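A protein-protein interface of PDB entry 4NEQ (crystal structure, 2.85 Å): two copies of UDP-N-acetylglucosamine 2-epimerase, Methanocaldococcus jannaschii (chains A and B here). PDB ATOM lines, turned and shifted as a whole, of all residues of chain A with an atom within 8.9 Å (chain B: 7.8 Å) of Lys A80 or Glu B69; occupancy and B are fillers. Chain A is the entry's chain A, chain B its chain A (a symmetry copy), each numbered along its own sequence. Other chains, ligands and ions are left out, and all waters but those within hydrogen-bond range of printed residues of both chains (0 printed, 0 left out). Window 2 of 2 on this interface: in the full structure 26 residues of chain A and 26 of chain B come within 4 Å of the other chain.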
ATOM      1  N   ILE A  33     -23.192 -20.478 -26.062  1.00  0.00           N
ATOM      2  CA  ILE A  33     -22.555 -21.403 -25.155  1.00  0.00           C
ATOM      3  C   ILE A  33     -22.715 -20.851 -23.750  1.00  0.00           C
ATOM      4  O   ILE A  33     -22.121 -19.822 -23.409  1.00  0.00           O
ATOM      5  CB  ILE A  33     -21.050 -21.561 -25.463  1.00  0.00           C
ATOM      6  CG1 ILE A  33     -20.816 -21.712 -26.968  1.00  0.00           C
ATOM      7  CG2 ILE A  33     -20.464 -22.734 -24.689  1.00  0.00           C
ATOM      8  CD1 ILE A  33     -19.374 -21.921 -27.334  1.00  0.00           C
ATOM      9  N   TYR A  58     -25.888 -24.990 -26.357  1.00  0.00           N
ATOM     10  CA  TYR A  58     -24.888 -25.662 -25.511  1.00  0.00           C
ATOM     11  C   TYR A  58     -24.852 -25.201 -24.067  1.00  0.00           C
ATOM     12  O   TYR A  58     -24.478 -24.069 -23.782  1.00  0.00           O
ATOM     13  CB  TYR A  58     -23.493 -25.408 -26.055  1.00  0.00           C
ATOM     14  CG  TYR A  58     -23.322 -25.890 -27.446  1.00  0.00           C
ATOM     15  CD1 TYR A  58     -23.111 -27.236 -27.707  1.00  0.00           C
ATOM     16  CD2 TYR A  58     -23.373 -25.013 -28.503  1.00  0.00           C
ATOM     17  CE1 TYR A  58     -22.954 -27.694 -28.983  1.00  0.00           C
ATOM     18  CE2 TYR A  58     -23.213 -25.453 -29.787  1.00  0.00           C
ATOM     19  CZ  TYR A  58     -23.015 -26.803 -30.029  1.00  0.00           C
ATOM     20  OH  TYR A  58     -22.858 -27.263 -31.318  1.00  0.00           O
ATOM     21  N   LEU A  60     -22.674 -26.061 -20.785  1.00  0.00           N
ATOM     22  CA  LEU A  60     -21.499 -26.755 -20.294  1.00  0.00           C
ATOM     23  C   LEU A  60     -21.445 -26.595 -18.800  1.00  0.00           C
ATOM     24  O   LEU A  60     -21.314 -25.486 -18.307  1.00  0.00           O
ATOM     25  CB  LEU A  60     -20.230 -26.149 -20.887  1.00  0.00           C
ATOM     26  CG  LEU A  60     -20.227 -25.907 -22.393  1.00  0.00           C
ATOM     27  CD1 LEU A  60     -18.894 -25.316 -22.807  1.00  0.00           C
ATOM     28  CD2 LEU A  60     -20.519 -27.200 -23.131  1.00  0.00           C
ATOM     29  N   THR A  71     -11.056 -22.398 -15.273  1.00  0.00           N
ATOM     30  CA  THR A  71     -10.564 -21.864 -16.533  1.00  0.00           C
ATOM     31  C   THR A  71     -10.108 -22.942 -17.521  1.00  0.00           C
ATOM     32  O   THR A  71     -10.426 -22.879 -18.702  1.00  0.00           O
ATOM     33  CB  THR A  71      -9.468 -20.846 -16.283  1.00  0.00           C
ATOM     34  OG1 THR A  71     -10.038 -19.723 -15.589  1.00  0.00           O
ATOM     35  CG2 THR A  71      -8.878 -20.382 -17.595  1.00  0.00           C
ATOM     36  N   GLY A  72      -9.399 -23.944 -17.029  1.00  0.00           N
ATOM     37  CA  GLY A  72      -8.938 -25.040 -17.859  1.00  0.00           C
ATOM     38  C   GLY A  72     -10.053 -25.892 -18.427  1.00  0.00           C
ATOM     39  O   GLY A  72     -10.047 -26.187 -19.626  1.00  0.00           O
ATOM     40  N   LYS A  73     -10.997 -26.312 -17.582  1.00  0.00           N
ATOM     41  CA  LYS A  73     -12.129 -27.099 -18.061  1.00  0.00           C
ATOM     42  C   LYS A  73     -12.924 -26.315 -19.121  1.00  0.00           C
ATOM     43  O   LYS A  73     -13.294 -26.872 -20.162  1.00  0.00           O
ATOM     44  CB  LYS A  73     -13.032 -27.559 -16.917  1.00  0.00           C
ATOM     45  CG  LYS A  73     -12.413 -28.616 -15.999  1.00  0.00           C
ATOM     46  CD  LYS A  73     -13.278 -28.871 -14.742  1.00  0.00           C
ATOM     47  CE  LYS A  73     -12.563 -29.765 -13.708  1.00  0.00           C
ATOM     48  NZ  LYS A  73     -13.126 -29.648 -12.320  1.00  0.00           N
ATOM     49  N   MET A  74     -13.160 -25.020 -18.914  1.00  0.00           N
ATOM     50  CA  MET A  74     -13.818 -24.322 -20.017  1.00  0.00           C
ATOM     51  C   MET A  74     -12.965 -24.137 -21.254  1.00  0.00           C
ATOM     52  O   MET A  74     -13.498 -24.157 -22.345  1.00  0.00           O
ATOM     53  CB  MET A  74     -14.498 -23.003 -19.639  1.00  0.00           C
ATOM     54  CG  MET A  74     -14.437 -22.648 -18.196  1.00  0.00           C
ATOM     55  SD  MET A  74     -15.639 -21.188 -17.701  1.00  0.00           S
ATOM     56  CE  MET A  74     -14.360 -20.258 -16.618  1.00  0.00           C
ATOM     57  N   LEU A  75     -11.662 -23.923 -21.103  1.00  0.00           N
ATOM     58  CA  LEU A  75     -10.770 -23.899 -22.267  1.00  0.00           C
ATOM     59  C   LEU A  75     -10.953 -25.168 -23.128  1.00  0.00           C
ATOM     60  O   LEU A  75     -11.204 -25.100 -24.339  1.00  0.00           O
ATOM     61  CB  LEU A  75      -9.332 -23.772 -21.812  1.00  0.00           C
ATOM     62  CG  LEU A  75      -8.629 -22.471 -22.157  1.00  0.00           C
ATOM     63  CD1 LEU A  75      -9.601 -21.343 -22.103  1.00  0.00           C
ATOM     64  CD2 LEU A  75      -7.507 -22.211 -21.170  1.00  0.00           C
ATOM     65  N   ILE A  76     -10.874 -26.324 -22.480  1.00  0.00           N
ATOM     66  CA  ILE A  76     -11.107 -27.596 -23.152  1.00  0.00           C
ATOM     67  C   ILE A  76     -12.511 -27.707 -23.796  1.00  0.00           C
ATOM     68  O   ILE A  76     -12.626 -27.982 -25.009  1.00  0.00           O
ATOM     69  CB  ILE A  76     -10.816 -28.763 -22.176  1.00  0.00           C
ATOM     70  CG1 ILE A  76      -9.302 -28.897 -21.974  1.00  0.00           C
ATOM     71  CG2 ILE A  76     -11.418 -30.069 -22.680  1.00  0.00           C
ATOM     72  CD1 ILE A  76      -8.821 -28.909 -20.526  1.00  0.00           C
ATOM     73  N   GLU A  77     -13.562 -27.463 -23.001  1.00  0.00           N
ATOM     74  CA  GLU A  77     -14.955 -27.662 -23.447  1.00  0.00           C
ATOM     75  C   GLU A  77     -15.422 -26.672 -24.524  1.00  0.00           C
ATOM     76  O   GLU A  77     -15.937 -27.069 -25.600  1.00  0.00           O
ATOM     77  CB  GLU A  77     -15.915 -27.630 -22.256  1.00  0.00           C
ATOM     78  CG  GLU A  77     -15.790 -28.817 -21.325  1.00  0.00           C
ATOM     79  CD  GLU A  77     -15.950 -30.140 -22.052  1.00  0.00           C
ATOM     80  OE1 GLU A  77     -16.886 -30.255 -22.875  1.00  0.00           O
ATOM     81  OE2 GLU A  77     -15.134 -31.061 -21.814  1.00  0.00           O
ATOM     82  N   ILE A  78     -15.246 -25.387 -24.224  1.00  0.00           N
ATOM     83  CA  ILE A  78     -15.468 -24.331 -25.201  1.00  0.00           C
ATOM     84  C   ILE A  78     -14.703 -24.635 -26.467  1.00  0.00           C
ATOM     85  O   ILE A  78     -15.226 -24.428 -27.560  1.00  0.00           O
ATOM     86  CB  ILE A  78     -15.089 -22.933 -24.669  1.00  0.00           C
ATOM     87  CG1 ILE A  78     -16.064 -22.521 -23.562  1.00  0.00           C
ATOM     88  CG2 ILE A  78     -15.107 -21.894 -25.792  1.00  0.00           C
ATOM     89  CD1 ILE A  78     -15.618 -21.333 -22.770  1.00  0.00           C
ATOM     90  N   GLU A  79     -13.488 -25.163 -26.334  1.00  0.00           N
ATOM     91  CA  GLU A  79     -12.752 -25.565 -27.536  1.00  0.00           C
ATOM     92  C   GLU A  79     -13.429 -26.665 -28.361  1.00  0.00           C
ATOM     93  O   GLU A  79     -13.422 -26.610 -29.593  1.00  0.00           O
ATOM     94  CB  GLU A  79     -11.329 -25.991 -27.220  1.00  0.00           C
ATOM     95  CG  GLU A  79     -10.526 -26.234 -28.457  1.00  0.00           C
ATOM     96  CD  GLU A  79      -9.191 -26.806 -28.140  1.00  0.00           C
ATOM     97  OE1 GLU A  79      -9.151 -27.905 -27.538  1.00  0.00           O
ATOM     98  OE2 GLU A  79      -8.193 -26.140 -28.474  1.00  0.00           O
ATOM     99  N   LYS A  80     -13.989 -27.670 -27.696  1.00  0.00           N
ATOM    100  CA  LYS A  80     -14.655 -28.732 -28.447  1.00  0.00           C
ATOM    101  C   LYS A  80     -15.856 -28.164 -29.211  1.00  0.00           C
ATOM    102  O   LYS A  80     -16.088 -28.486 -30.403  1.00  0.00           O
ATOM    103  CB  LYS A  80     -15.057 -29.881 -27.531  1.00  0.00           C
ATOM    104  CG  LYS A  80     -13.930 -30.853 -27.235  1.00  0.00           C
ATOM    105  CD  LYS A  80     -14.053 -31.434 -25.833  1.00  0.00           C
ATOM    106  CE  LYS A  80     -13.077 -32.592 -25.655  1.00  0.00           C
ATOM    107  NZ  LYS A  80     -11.771 -32.331 -26.346  1.00  0.00           N
ATOM    108  N   VAL A  81     -16.601 -27.275 -28.556  1.00  0.00           N
ATOM    109  CA  VAL A  81     -17.679 -26.610 -29.288  1.00  0.00           C
ATOM    110  C   VAL A  81     -17.174 -25.758 -30.464  1.00  0.00           C
ATOM    111  O   VAL A  81     -17.668 -25.884 -31.556  1.00  0.00           O
ATOM    112  CB  VAL A  81     -18.595 -25.757 -28.393  1.00  0.00           C
ATOM    113  CG1 VAL A  81     -19.581 -24.999 -29.262  1.00  0.00           C
ATOM    114  CG2 VAL A  81     -19.334 -26.615 -27.387  1.00  0.00           C
ATOM    115  N   LEU A  82     -16.189 -24.896 -30.258  1.00  0.00           N
ATOM    116  CA  LEU A  82     -15.803 -24.010 -31.348  1.00  0.00           C
ATOM    117  C   LEU A  82     -15.139 -24.758 -32.503  1.00  0.00           C
ATOM    118  O   LEU A  82     -15.176 -24.312 -33.650  1.00  0.00           O
ATOM    119  CB  LEU A  82     -14.938 -22.847 -30.856  1.00  0.00           C
ATOM    120  CG  LEU A  82     -15.597 -21.895 -29.849  1.00  0.00           C
ATOM    121  CD1 LEU A  82     -14.825 -20.593 -29.783  1.00  0.00           C
ATOM    122  CD2 LEU A  82     -17.051 -21.635 -30.184  1.00  0.00           C
ATOM    123  N   LEU A  83     -14.533 -25.899 -32.203  1.00  0.00           N
ATOM    124  CA  LEU A  83     -14.040 -26.768 -33.269  1.00  0.00           C
ATOM    125  C   LEU A  83     -15.208 -27.325 -34.061  1.00  0.00           C
ATOM    126  O   LEU A  83     -15.177 -27.306 -35.284  1.00  0.00           O
ATOM    127  CB  LEU A  83     -13.199 -27.917 -32.728  1.00  0.00           C
ATOM    128  CG  LEU A  83     -11.825 -27.550 -32.210  1.00  0.00           C
ATOM    129  CD1 LEU A  83     -11.117 -28.812 -31.832  1.00  0.00           C
ATOM    130  CD2 LEU A  83     -11.061 -26.780 -33.245  1.00  0.00           C
ATOM    131  N   LYS A  84     -16.234 -27.822 -33.371  1.00  0.00           N
ATOM    132  CA  LYS A  84     -17.453 -28.255 -34.074  1.00  0.00           C
ATOM    133  C   LYS A  84     -18.196 -27.135 -34.858  1.00  0.00           C
ATOM    134  O   LYS A  84     -18.501 -27.300 -36.032  1.00  0.00           O
ATOM    135  CB  LYS A  84     -18.398 -28.939 -33.087  1.00  0.00           C
ATOM    136  CG  LYS A  84     -19.633 -29.587 -33.679  1.00  0.00           C
ATOM    137  CD  LYS A  84     -20.448 -30.249 -32.560  1.00  0.00           C
ATOM    138  CE  LYS A  84     -19.538 -31.083 -31.626  1.00  0.00           C
ATOM    139  NZ  LYS A  84     -20.286 -31.771 -30.528  1.00  0.00           N
ATOM    140  N   GLU A  85     -18.467 -25.999 -34.214  1.00  0.00           N
ATOM    141  CA  GLU A  85     -19.304 -24.934 -34.782  1.00  0.00           C
ATOM    142  C   GLU A  85     -18.611 -24.037 -35.787  1.00  0.00           C
ATOM    143  O   GLU A  85     -19.260 -23.502 -36.678  1.00  0.00           O
ATOM    144  CB  GLU A  85     -19.882 -24.043 -33.683  1.00  0.00           C
ATOM    145  CG  GLU A  85     -20.833 -24.735 -32.748  1.00  0.00           C
ATOM    146  CD  GLU A  85     -22.208 -24.902 -33.321  1.00  0.00           C
ATOM    147  OE1 GLU A  85     -22.466 -24.437 -34.455  1.00  0.00           O
ATOM    148  OE2 GLU A  85     -23.039 -25.503 -32.628  1.00  0.00           O
ATOM    149  N   LYS A  86     -17.308 -23.860 -35.623  1.00  0.00           N
ATOM    150  CA  LYS A  86     -16.511 -23.021 -36.515  1.00  0.00           C
ATOM    151  C   LYS A  86     -17.168 -21.683 -36.876  1.00  0.00           C
ATOM    152  O   LYS A  86     -17.478 -21.444 -38.039  1.00  0.00           O
ATOM    153  CB  LYS A  86     -16.161 -23.774 -37.808  1.00  0.00           C
ATOM    154  CG  LYS A  86     -15.705 -25.205 -37.628  1.00  0.00           C
ATOM    155  CD  LYS A  86     -16.696 -26.215 -38.244  1.00  0.00           C
ATOM    156  CE  LYS A  86     -16.114 -27.654 -38.242  1.00  0.00           C
ATOM    157  NZ  LYS A  86     -17.067 -28.755 -38.612  1.00  0.00           N
ATOM    158  N   PRO A  87     -17.385 -20.807 -35.886  1.00  0.00           N
ATOM    159  CA  PRO A  87     -17.956 -19.498 -36.221  1.00  0.00           C
ATOM    160  C   PRO A  87     -16.903 -18.509 -36.722  1.00  0.00           C
ATOM    161  O   PRO A  87     -15.711 -18.820 -36.739  1.00  0.00           O
ATOM    162  CB  PRO A  87     -18.494 -19.022 -34.879  1.00  0.00           C
ATOM    163  CG  PRO A  87     -17.532 -19.612 -33.894  1.00  0.00           C
ATOM    164  CD  PRO A  87     -17.204 -20.974 -34.430  1.00  0.00           C
ATOM    165  N   VAL A 105      -9.585 -19.294 -26.012  1.00  0.00           N
ATOM    166  CA  VAL A 105      -9.882 -20.293 -27.045  1.00  0.00           C
ATOM    167  C   VAL A 105     -10.117 -19.710 -28.453  1.00  0.00           C
ATOM    168  O   VAL A 105      -9.499 -20.152 -29.437  1.00  0.00           O
ATOM    169  CB  VAL A 105     -11.113 -21.117 -26.719  1.00  0.00           C
ATOM    170  CG1 VAL A 105     -11.154 -22.339 -27.617  1.00  0.00           C
ATOM    171  CG2 VAL A 105     -11.080 -21.532 -25.300  1.00  0.00           C
ATOM    172  N   LYS A 108      -7.002 -18.523 -29.981  1.00  0.00           N
ATOM    173  CA  LYS A 108      -6.050 -19.536 -30.398  1.00  0.00           C
ATOM    174  C   LYS A 108      -6.532 -20.325 -31.613  1.00  0.00           C
ATOM    175  O   LYS A 108      -5.714 -20.843 -32.374  1.00  0.00           O
ATOM    176  CB  LYS A 108      -5.671 -20.443 -29.234  1.00  0.00           C
ATOM    177  CG  LYS A 108      -4.627 -19.801 -28.337  1.00  0.00           C
ATOM    178  CD  LYS A 108      -4.461 -20.566 -27.016  1.00  0.00           C
ATOM    179  CE  LYS A 108      -3.224 -20.091 -26.259  1.00  0.00           C
ATOM    180  NZ  LYS A 108      -2.948 -21.075 -25.209  1.00  0.00           N
ATOM    181  N   LEU A 109      -7.850 -20.394 -31.803  1.00  0.00           N
ATOM    182  CA  LEU A 109      -8.439 -21.006 -33.000  1.00  0.00           C
ATOM    183  C   LEU A 109      -8.514 -20.016 -34.166  1.00  0.00           C
ATOM    184  O   LEU A 109      -9.085 -20.305 -35.211  1.00  0.00           O
ATOM    185  CB  LEU A 109      -9.827 -21.550 -32.701  1.00  0.00           C
ATOM    186  CG  LEU A 109      -9.838 -22.746 -31.777  1.00  0.00           C
ATOM    187  CD1 LEU A 109     -11.206 -23.384 -31.752  1.00  0.00           C
ATOM    188  CD2 LEU A 109      -8.825 -23.689 -32.295  1.00  0.00           C
ATOM    189  N   ILE B  62       2.832 -32.355 -20.134  1.00  0.00           N
ATOM    190  CA  ILE B  62       1.547 -31.828 -20.537  1.00  0.00           C
ATOM    191  C   ILE B  62       1.009 -32.764 -21.613  1.00  0.00           C
ATOM    192  O   ILE B  62      -0.197 -32.819 -21.896  1.00  0.00           O
ATOM    193  CB  ILE B  62       1.702 -30.385 -21.040  1.00  0.00           C
ATOM    194  CG1 ILE B  62       2.185 -29.492 -19.892  1.00  0.00           C
ATOM    195  CG2 ILE B  62       0.409 -29.855 -21.599  1.00  0.00           C
ATOM    196  CD1 ILE B  62       1.428 -29.680 -18.570  1.00  0.00           C
ATOM    197  N   GLY B  63       1.930 -33.532 -22.185  1.00  0.00           N
ATOM    198  CA  GLY B  63       1.626 -34.406 -23.293  1.00  0.00           C
ATOM    199  C   GLY B  63       1.239 -33.533 -24.458  1.00  0.00           C
ATOM    200  O   GLY B  63       1.315 -32.312 -24.370  1.00  0.00           O
ATOM    201  N   SER B  64       0.836 -34.146 -25.562  1.00  0.00           N
ATOM    202  CA  SER B  64       0.260 -33.363 -26.635  1.00  0.00           C
ATOM    203  C   SER B  64      -1.258 -33.489 -26.582  1.00  0.00           C
ATOM    204  O   SER B  64      -1.809 -34.270 -25.798  1.00  0.00           O
ATOM    205  CB  SER B  64       0.833 -33.756 -27.999  1.00  0.00           C
ATOM    206  OG  SER B  64       1.935 -32.920 -28.339  1.00  0.00           O
ATOM    207  N   GLY B  65      -1.917 -32.697 -27.417  1.00  0.00           N
ATOM    208  CA  GLY B  65      -3.356 -32.556 -27.420  1.00  0.00           C
ATOM    209  C   GLY B  65      -3.558 -31.170 -27.987  1.00  0.00           C
ATOM    210  O   GLY B  65      -2.585 -30.549 -28.426  1.00  0.00           O
ATOM    211  N   THR B  66      -4.789 -30.674 -27.970  1.00  0.00           N
ATOM    212  CA  THR B  66      -5.098 -29.372 -28.575  1.00  0.00           C
ATOM    213  C   THR B  66      -4.537 -28.155 -27.834  1.00  0.00           C
ATOM    214  O   THR B  66      -4.259 -28.229 -26.640  1.00  0.00           O
ATOM    215  CB  THR B  66      -6.598 -29.177 -28.672  1.00  0.00           C
ATOM    216  OG1 THR B  66      -7.262 -30.409 -28.371  1.00  0.00           O
ATOM    217  CG2 THR B  66      -6.966 -28.722 -30.058  1.00  0.00           C
ATOM    218  N   HIS B  67      -4.390 -27.036 -28.546  1.00  0.00           N
ATOM    219  CA  HIS B  67      -4.005 -25.752 -27.940  1.00  0.00           C
ATOM    220  C   HIS B  67      -4.732 -25.465 -26.617  1.00  0.00           C
ATOM    221  O   HIS B  67      -4.106 -25.206 -25.565  1.00  0.00           O
ATOM    222  CB  HIS B  67      -4.296 -24.620 -28.914  1.00  0.00           C
ATOM    223  CG  HIS B  67      -3.141 -24.267 -29.793  1.00  0.00           C
ATOM    224  ND1 HIS B  67      -1.853 -24.147 -29.314  1.00  0.00           N
ATOM    225  CD2 HIS B  67      -3.078 -23.999 -31.120  1.00  0.00           C
ATOM    226  CE1 HIS B  67      -1.046 -23.821 -30.309  1.00  0.00           C
ATOM    227  NE2 HIS B  67      -1.766 -23.725 -31.415  1.00  0.00           N
ATOM    228  N   GLY B  68      -6.058 -25.513 -26.698  1.00  0.00           N
ATOM    229  CA  GLY B  68      -6.935 -25.451 -25.548  1.00  0.00           C
ATOM    230  C   GLY B  68      -6.561 -26.417 -24.450  1.00  0.00           C
ATOM    231  O   GLY B  68      -6.359 -25.979 -23.323  1.00  0.00           O
ATOM    232  N   GLU B  69      -6.453 -27.714 -24.742  1.00  0.00           N
ATOM    233  CA  GLU B  69      -6.101 -28.650 -23.667  1.00  0.00           C
ATOM    234  C   GLU B  69      -4.670 -28.518 -23.184  1.00  0.00           C
ATOM    235  O   GLU B  69      -4.369 -28.877 -22.053  1.00  0.00           O
ATOM    236  CB  GLU B  69      -6.378 -30.116 -24.003  1.00  0.00           C
ATOM    237  CG  GLU B  69      -7.040 -30.368 -25.314  1.00  0.00           C
ATOM    238  CD  GLU B  69      -7.250 -31.851 -25.558  1.00  0.00           C
ATOM    239  OE1 GLU B  69      -8.209 -32.418 -24.971  1.00  0.00           O
ATOM    240  OE2 GLU B  69      -6.452 -32.443 -26.326  1.00  0.00           O
ATOM    241  N   GLN B  70      -3.771 -28.034 -24.029  1.00  0.00           N
ATOM    242  CA  GLN B  70      -2.403 -27.871 -23.572  1.00  0.00           C
ATOM    243  C   GLN B  70      -2.432 -26.831 -22.487  1.00  0.00           C
ATOM    244  O   GLN B  70      -2.043 -27.094 -21.346  1.00  0.00           O
ATOM    245  CB  GLN B  70      -1.468 -27.470 -24.713  1.00  0.00           C
ATOM    246  CG  GLN B  70      -1.284 -28.561 -25.762  1.00  0.00           C
ATOM    247  CD  GLN B  70      -0.976 -29.932 -25.162  1.00  0.00           C
ATOM    248  OE1 GLN B  70      -1.861 -30.631 -24.642  1.00  0.00           O
ATOM    249  NE2 GLN B  70       0.286 -30.326 -25.244  1.00  0.00           N
ATOM    250  N   THR B  71      -2.983 -25.674 -22.839  1.00  0.00           N
ATOM    251  CA  THR B  71      -3.112 -24.571 -21.900  1.00  0.00           C
ATOM    252  C   THR B  71      -3.887 -24.933 -20.630  1.00  0.00           C
ATOM    253  O   THR B  71      -3.478 -24.584 -19.529  1.00  0.00           O
ATOM    254  CB  THR B  71      -3.712 -23.359 -22.587  1.00  0.00           C
ATOM    255  OG1 THR B  71      -2.791 -22.899 -23.591  1.00  0.00           O
ATOM    256  CG2 THR B  71      -3.954 -22.256 -21.582  1.00  0.00           C
ATOM    257  N   GLY B  72      -4.981 -25.660 -20.783  1.00  0.00           N
ATOM    258  CA  GLY B  72      -5.781 -26.093 -19.654  1.00  0.00           C
ATOM    259  C   GLY B  72      -5.070 -27.059 -18.730  1.00  0.00           C
ATOM    260  O   GLY B  72      -5.100 -26.871 -17.510  1.00  0.00           O
ATOM    261  N   LYS B  73      -4.451 -28.100 -19.288  1.00  0.00           N
ATOM    262  CA  LYS B  73      -3.705 -29.050 -18.469  1.00  0.00           C
ATOM    263  C   LYS B  73      -2.576 -28.336 -17.703  1.00  0.00           C
ATOM    264  O   LYS B  73      -2.383 -28.578 -16.505  1.00  0.00           O
ATOM    265  CB  LYS B  73      -3.163 -30.217 -19.294  1.00  0.00           C
ATOM    266  CG  LYS B  73      -4.230 -31.181 -19.817  1.00  0.00           C
ATOM    267  CD  LYS B  73      -3.649 -32.200 -20.823  1.00  0.00           C
ATOM    268  CE  LYS B  73      -4.747 -33.031 -21.519  1.00  0.00           C
ATOM    269  NZ  LYS B  73      -4.298 -33.664 -22.807  1.00  0.00           N
ATOM    270  N   MET B  74      -1.849 -27.420 -18.343  1.00  0.00           N
ATOM    271  CA  MET B  74      -0.878 -26.706 -17.517  1.00  0.00           C
ATOM    272  C   MET B  74      -1.479 -25.758 -16.501  1.00  0.00           C
ATOM    273  O   MET B  74      -0.915 -25.599 -15.438  1.00  0.00           O
ATOM    274  CB  MET B  74       0.249 -26.014 -18.288  1.00  0.00           C
ATOM    275  CG  MET B  74       0.223 -26.210 -19.762  1.00  0.00           C
ATOM    276  SD  MET B  74       1.873 -25.655 -20.652  1.00  0.00           S
ATOM    277  CE  MET B  74       1.003 -24.743 -22.096  1.00  0.00           C
ATOM    278  N   LEU B  75      -2.588 -25.100 -16.822  1.00  0.00           N
ATOM    279  CA  LEU B  75      -3.297 -24.297 -15.821  1.00  0.00           C
ATOM    280  C   LEU B  75      -3.580 -25.125 -14.549  1.00  0.00           C
ATOM    281  O   LEU B  75      -3.227 -24.735 -13.428  1.00  0.00           O
ATOM    282  CB  LEU B  75      -4.589 -23.767 -16.405  1.00  0.00           C
ATOM    283  CG  LEU B  75      -4.669 -22.264 -16.609  1.00  0.00           C
ATOM    284  CD1 LEU B  75      -3.329 -21.734 -16.988  1.00  0.00           C
ATOM    285  CD2 LEU B  75      -5.662 -21.943 -17.709  1.00  0.00           C
ATOM    286  N   ILE B  76      -4.175 -26.296 -14.741  1.00  0.00           N
ATOM    287  CA  ILE B  76      -4.429 -27.215 -13.640  1.00  0.00           C
ATOM    288  C   ILE B  76      -3.146 -27.651 -12.889  1.00  0.00           C
ATOM    289  O   ILE B  76      -3.057 -27.491 -11.653  1.00  0.00           O
ATOM    290  CB  ILE B  76      -5.248 -28.428 -14.150  1.00  0.00           C
ATOM    291  CG1 ILE B  76      -6.696 -27.993 -14.411  1.00  0.00           C
ATOM    292  CG2 ILE B  76      -5.194 -29.586 -13.163  1.00  0.00           C
ATOM    293  CD1 ILE B  76      -7.254 -28.329 -15.790  1.00  0.00           C
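Among the printed residues, merely in contact across the chains: Thr A71 with Leu B75 (3.6 Å), Leu A75 with Thr B71 (3.6 Å), Ile A76 with Glu B69 (3.6 Å), Gly A72 with Gly B72 (3.8 Å), Glu A79 with Glu B69 (3.9 Å), Glu A79 with His B67 (3.9 Å), Leu A75 with Leu B75 (3.9 Å) and Leu A75 with Gly B68 (3.999 Å).
Printed residues of chain B that touch a printed residue of chain A: Thr B66, His B67, Gly B68, Glu B69, Thr B71, Gly B72 and Leu B75.
Hydrophobic or aromatic side chains of chain B within 4 Å of the printed part of chain A: Leu B75.
Printed residues of chain A that touch a printed residue of chain B: Thr A71, Gly A72, Leu A75, Ile A76, Glu A79, Lys A80 and Lys A108.
Hydrophobic or aromatic side chains of chain A that line the printed part of chain B: Leu A75 and Ile A76.
Among the printed residues, 12 pairs touch across the chains.
Among the printed residues, Asp or Glu carboxylates within 4 Å of a Lys or Arg side-chain nitrogen of the other chain: Lys A80 with Glu B69.
The backbone NH of Thr B66 is in hydrogen-bond range of the side-chain carboxylate of Glu B69 (2.9 Å).
The backbone carbonyl oxygen of His B67 lies within hydrogen-bond range of the side-chain hydroxyl of Thr B71 (3.3 Å).
Thr A71 touches Leu B75, and with the chains exchanged Leu A75 touches Thr B71.
Gly A72 touches its own counterpart, Gly B72.
Leu B75 touches its own counterpart, Leu A75.
Positions printed for both chains: 71, 72, 73, 74, 75 and 76.
Of the 12 pairs that touch across the chains among the printed residues, 4 have their exchanged pair printed and touching as well.
The side-chain carboxylate (OE1) of Glu A79 sits close to the side-chain hydroxyl (OG1) of Thr B66.
The backbone NH (N) of Gly B68 is in hydrogen-bond range of the side-chain carboxylate (OE2) of Glu A79.
NZ of Lys A80 lies within salt-bridge range of OE1 of Glu B69, 3.8 Å away.
The side-chain amino group of Lys A108 lies within hydrogen-bond range of the side-chain hydroxyl of Thr B71, at 2.4 Å.
Lys A80 touches just one residue of chain B: Glu B69 (3.8 Å).
No residue of chain A comes within 4 Å of Gly B65.
Of the printed residues of chain A, Gly B68 touches Leu A75 (3.999 Å) and Glu A79 (2.8 Å).
Printed residues of chain B within 4 Å of Gly A72: Gly B72 (3.8 Å).
Val A105 touches none of the printed residues of chain B.
The nearest residue of chain B that does not touch Lys A80 is Thr B66 (5.3 Å).
The nearest printed residue of chain A that does not touch Gly B72 is Ile A76 (4.2 Å).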
